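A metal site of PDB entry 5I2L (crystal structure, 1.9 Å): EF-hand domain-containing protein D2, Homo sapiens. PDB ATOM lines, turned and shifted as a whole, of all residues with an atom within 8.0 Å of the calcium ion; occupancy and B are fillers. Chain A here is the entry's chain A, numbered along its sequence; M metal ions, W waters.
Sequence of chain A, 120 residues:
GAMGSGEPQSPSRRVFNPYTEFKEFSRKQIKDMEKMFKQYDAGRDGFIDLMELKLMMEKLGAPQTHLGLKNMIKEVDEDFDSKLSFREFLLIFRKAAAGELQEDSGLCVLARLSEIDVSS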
ATOM      1  N   PHE A  37      -6.282  -3.428  -6.872  1.00  0.00           N
ATOM      2  CA  PHE A  37      -4.818  -3.335  -7.009  1.00  0.00           C
ATOM      3  C   PHE A  37      -4.155  -4.555  -6.386  1.00  0.00           C
ATOM      4  O   PHE A  37      -3.310  -5.226  -7.003  1.00  0.00           O
ATOM      5  CB  PHE A  37      -4.313  -2.064  -6.294  1.00  0.00           C
ATOM      6  CG  PHE A  37      -2.837  -1.808  -6.466  1.00  0.00           C
ATOM      7  CD1 PHE A  37      -2.337  -1.206  -7.617  1.00  0.00           C
ATOM      8  CD2 PHE A  37      -1.934  -2.157  -5.458  1.00  0.00           C
ATOM      9  CE1 PHE A  37      -0.976  -0.961  -7.752  1.00  0.00           C
ATOM     10  CE2 PHE A  37      -0.568  -1.922  -5.602  1.00  0.00           C
ATOM     11  CZ  PHE A  37      -0.089  -1.316  -6.747  1.00  0.00           C
ATOM     12  N   TYR A  40      -4.430  -7.908  -8.244  1.00  0.00           N
ATOM     13  CA  TYR A  40      -3.602  -8.137  -9.404  1.00  0.00           C
ATOM     14  C   TYR A  40      -2.101  -7.943  -9.193  1.00  0.00           C
ATOM     15  O   TYR A  40      -1.312  -8.286 -10.062  1.00  0.00           O
ATOM     16  CB  TYR A  40      -4.151  -7.363 -10.605  1.00  0.00           C
ATOM     17  CG  TYR A  40      -5.513  -7.887 -11.015  1.00  0.00           C
ATOM     18  CD1 TYR A  40      -5.628  -9.047 -11.766  1.00  0.00           C
ATOM     19  CD2 TYR A  40      -6.680  -7.227 -10.646  1.00  0.00           C
ATOM     20  CE1 TYR A  40      -6.863  -9.549 -12.128  1.00  0.00           C
ATOM     21  CE2 TYR A  40      -7.926  -7.711 -11.012  1.00  0.00           C
ATOM     22  CZ  TYR A  40      -8.009  -8.877 -11.761  1.00  0.00           C
ATOM     23  OH  TYR A  40      -9.235  -9.365 -12.133  1.00  0.00           O
ATOM     24  N   ASP A  41      -1.710  -7.420  -8.034  1.00  0.00           N
ATOM     25  CA  ASP A  41      -0.307  -7.419  -7.637  1.00  0.00           C
ATOM     26  C   ASP A  41       0.052  -8.828  -7.125  1.00  0.00           C
ATOM     27  O   ASP A  41       0.212  -9.055  -5.920  1.00  0.00           O
ATOM     28  CB  ASP A  41      -0.016  -6.344  -6.573  1.00  0.00           C
ATOM     29  CG  ASP A  41       1.379  -6.458  -5.977  1.00  0.00           C
ATOM     30  OD1 ASP A  41       2.176  -7.240  -6.501  1.00  0.00           O
ATOM     31  OD2 ASP A  41       1.680  -5.827  -4.941  1.00  0.00           O
ATOM     32  N   ALA A  42       0.183  -9.756  -8.066  1.00  0.00           N
ATOM     33  CA  ALA A  42       0.412 -11.162  -7.765  1.00  0.00           C
ATOM     34  C   ALA A  42       1.658 -11.387  -6.933  1.00  0.00           C
ATOM     35  O   ALA A  42       1.717 -12.333  -6.143  1.00  0.00           O
ATOM     36  CB  ALA A  42       0.486 -11.971  -9.057  1.00  0.00           C
ATOM     37  N   GLY A  43       2.654 -10.523  -7.097  1.00  0.00           N
ATOM     38  CA  GLY A  43       3.922 -10.688  -6.395  1.00  0.00           C
ATOM     39  C   GLY A  43       3.998 -10.055  -5.017  1.00  0.00           C
ATOM     40  O   GLY A  43       4.991 -10.234  -4.311  1.00  0.00           O
ATOM     41  N   ARG A  44       2.957  -9.301  -4.635  1.00  0.00           N
ATOM     42  CA  ARG A  44       2.861  -8.650  -3.330  1.00  0.00           C
ATOM     43  C   ARG A  44       4.012  -7.682  -3.017  1.00  0.00           C
ATOM     44  O   ARG A  44       4.369  -7.494  -1.850  1.00  0.00           O
ATOM     45  CB  ARG A  44       2.715  -9.673  -2.194  1.00  0.00           C
ATOM     46  CG  ARG A  44       1.624 -10.721  -2.410  1.00  0.00           C
ATOM     47  CD  ARG A  44       1.388 -11.581  -1.165  1.00  0.00           C
ATOM     48  NE  ARG A  44       2.608 -12.227  -0.673  1.00  0.00           N
ATOM     49  CZ  ARG A  44       2.973 -13.460  -0.995  1.00  0.00           C
ATOM     50  NH1 ARG A  44       2.216 -14.189  -1.803  1.00  0.00           N
ATOM     51  NH2 ARG A  44       4.097 -13.981  -0.492  1.00  0.00           N
ATOM     52  N   ASP A  45       4.577  -7.064  -4.048  1.00  0.00           N
ATOM     53  CA  ASP A  45       5.665  -6.108  -3.846  1.00  0.00           C
ATOM     54  C   ASP A  45       5.168  -4.659  -3.787  1.00  0.00           C
ATOM     55  O   ASP A  45       5.946  -3.731  -3.595  1.00  0.00           O
ATOM     56  CB  ASP A  45       6.763  -6.251  -4.914  1.00  0.00           C
ATOM     57  CG  ASP A  45       6.297  -5.876  -6.285  1.00  0.00           C
ATOM     58  OD1 ASP A  45       5.082  -5.797  -6.440  1.00  0.00           O
ATOM     59  OD2 ASP A  45       7.105  -5.639  -7.203  1.00  0.00           O
ATOM     60  N   GLY A  46       3.863  -4.479  -3.980  1.00  0.00           N
ATOM     61  CA  GLY A  46       3.300  -3.126  -3.920  1.00  0.00           C
ATOM     62  C   GLY A  46       3.212  -2.379  -5.247  1.00  0.00           C
ATOM     63  O   GLY A  46       2.989  -1.178  -5.266  1.00  0.00           O
ATOM     64  N   PHE A  47       3.406  -3.094  -6.359  1.00  0.00           N
ATOM     65  CA  PHE A  47       3.358  -2.466  -7.679  1.00  0.00           C
ATOM     66  C   PHE A  47       2.632  -3.370  -8.626  1.00  0.00           C
ATOM     67  O   PHE A  47       2.527  -4.551  -8.388  1.00  0.00           O
ATOM     68  CB  PHE A  47       4.771  -2.275  -8.229  1.00  0.00           C
ATOM     69  CG  PHE A  47       5.648  -1.447  -7.350  1.00  0.00           C
ATOM     70  CD1 PHE A  47       5.572  -0.065  -7.393  1.00  0.00           C
ATOM     71  CD2 PHE A  47       6.544  -2.043  -6.479  1.00  0.00           C
ATOM     72  CE1 PHE A  47       6.352   0.714  -6.571  1.00  0.00           C
ATOM     73  CE2 PHE A  47       7.349  -1.264  -5.655  1.00  0.00           C
ATOM     74  CZ  PHE A  47       7.254   0.108  -5.710  1.00  0.00           C
ATOM     75  N   ILE A  48       2.110  -2.814  -9.699  1.00  0.00           N
ATOM     76  CA  ILE A  48       1.619  -3.647 -10.780  1.00  0.00           C
ATOM     77  C   ILE A  48       2.514  -3.387 -11.974  1.00  0.00           C
ATOM     78  O   ILE A  48       2.563  -2.267 -12.501  1.00  0.00           O
ATOM     79  CB  ILE A  48       0.149  -3.343 -11.121  1.00  0.00           C
ATOM     80  CG1 ILE A  48      -0.735  -3.901 -10.023  1.00  0.00           C
ATOM     81  CG2 ILE A  48      -0.240  -3.992 -12.455  1.00  0.00           C
ATOM     82  CD1 ILE A  48      -2.200  -3.650 -10.259  1.00  0.00           C
ATOM     83  N   ASP A  49       3.222  -4.430 -12.399  1.00  0.00           N
ATOM     84  CA  ASP A  49       4.116  -4.317 -13.547  1.00  0.00           C
ATOM     85  C   ASP A  49       3.394  -4.693 -14.840  1.00  0.00           C
ATOM     86  O   ASP A  49       2.176  -4.913 -14.851  1.00  0.00           O
ATOM     87  CB  ASP A  49       5.400  -5.182 -13.360  1.00  0.00           C
ATOM     88  CG  ASP A  49       5.116  -6.658 -13.173  1.00  0.00           C
ATOM     89  OD1 ASP A  49       4.091  -7.178 -13.699  1.00  0.00           O
ATOM     90  OD2 ASP A  49       5.930  -7.325 -12.495  1.00  0.00           O
ATOM     91  N   LEU A  50       4.145  -4.791 -15.927  1.00  0.00           N
ATOM     92  CA  LEU A  50       3.512  -4.931 -17.236  1.00  0.00           C
ATOM     93  C   LEU A  50       2.783  -6.251 -17.389  1.00  0.00           C
ATOM     94  O   LEU A  50       1.655  -6.320 -17.903  1.00  0.00           O
ATOM     95  CB  LEU A  50       4.543  -4.758 -18.371  1.00  0.00           C
ATOM     96  CG  LEU A  50       3.969  -4.963 -19.776  1.00  0.00           C
ATOM     97  CD1 LEU A  50       2.933  -3.940 -20.061  1.00  0.00           C
ATOM     98  CD2 LEU A  50       5.081  -4.843 -20.776  1.00  0.00           C
ATOM     99  N   GLU A  52       1.702  -8.186 -14.955  1.00  0.00           N
ATOM    100  CA  GLU A  52       0.560  -8.219 -14.056  1.00  0.00           C
ATOM    101  C   GLU A  52      -0.629  -7.468 -14.645  1.00  0.00           C
ATOM    102  O   GLU A  52      -1.782  -7.904 -14.531  1.00  0.00           O
ATOM    103  CB  GLU A  52       0.955  -7.669 -12.700  1.00  0.00           C
ATOM    104  CG  GLU A  52       1.751  -8.689 -11.929  1.00  0.00           C
ATOM    105  CD  GLU A  52       2.358  -8.085 -10.714  1.00  0.00           C
ATOM    106  OE1 GLU A  52       2.656  -6.881 -10.801  1.00  0.00           O
ATOM    107  OE2 GLU A  52       2.541  -8.796  -9.697  1.00  0.00           O
ATOM    108  N   LYS A  83       6.367   0.586 -13.773  1.00  0.00           N
ATOM    109  CA  LYS A  83       5.379  -0.234 -13.095  1.00  0.00           C
ATOM    110  C   LYS A  83       4.487   0.708 -12.297  1.00  0.00           C
ATOM    111  O   LYS A  83       4.812   1.849 -12.177  1.00  0.00           O
ATOM    112  CB  LYS A  83       6.044  -1.260 -12.179  1.00  0.00           C
ATOM    113  CG  LYS A  83       6.984  -0.654 -11.125  1.00  0.00           C
ATOM    114  CD  LYS A  83       7.759  -1.756 -10.390  1.00  0.00           C
ATOM    115  CE  LYS A  83       8.796  -1.106  -9.439  1.00  0.00           C
ATOM    116  NZ  LYS A  83       9.379  -2.144  -8.557  1.00  0.00           N
ATOM    117  N   LEU A  84       3.362   0.249 -11.763  1.00  0.00           N
ATOM    118  CA  LEU A  84       2.408   1.164 -11.116  1.00  0.00           C
ATOM    119  C   LEU A  84       2.384   0.983  -9.607  1.00  0.00           C
ATOM    120  O   LEU A  84       2.156  -0.112  -9.129  1.00  0.00           O
ATOM    121  CB  LEU A  84       1.007   0.910 -11.650  1.00  0.00           C
ATOM    122  CG  LEU A  84       0.813   1.072 -13.151  1.00  0.00           C
ATOM    123  CD1 LEU A  84      -0.612   0.755 -13.542  1.00  0.00           C
ATOM    124  CD2 LEU A  84       1.182   2.475 -13.557  1.00  0.00           C
HETATM  125 CA    CA M   1       3.823  -6.748  -8.438  1.00  0.00          CA
HETATM  126  O   HOH W   1       5.533  -8.541  -8.403  1.00  0.00           O
HETATM  127  O   HOH W   2       5.782  -5.593  -9.557  1.00  0.00           O
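OD1 of Asp 41 sits close to N of Gly 43 (3.4 Å).
The side-chain carboxylate (OD2) of Asp 41 lies within hydrogen-bond range of the backbone NH (N) of Gly 46 (2.7 Å).
N of Ala 42 sits close to OE2 of Glu 52, at 3.0 Å.
The backbone NH (N) of Glu 52 is in hydrogen-bond range of the side-chain carboxylate (OD1) of Asp 49, 2.9 Å away.
OE2 of Glu 52 sits close to N of Gly 43 (3.1 Å).
The side-chain carboxylate (OD1) of Asp 41 lies close to the backbone NH (N) of Arg 44, 2.9 Å away.
The calcium ion is bound by water W1, water W2, OD1 of Asp 45, O of Phe 47, OD1 of Asp 41, OE1 of Glu 52 and OE2 of Glu 52.
The calcium ion has seven donor atoms within binding distance.
Of the 15 residues printed, 4 come within 4 Å of the calcium ion.
Water W2 lies within hydrogen-bond range of the side-chain carboxylate of Asp 45 and the side-chain carboxylate of Asp 49.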
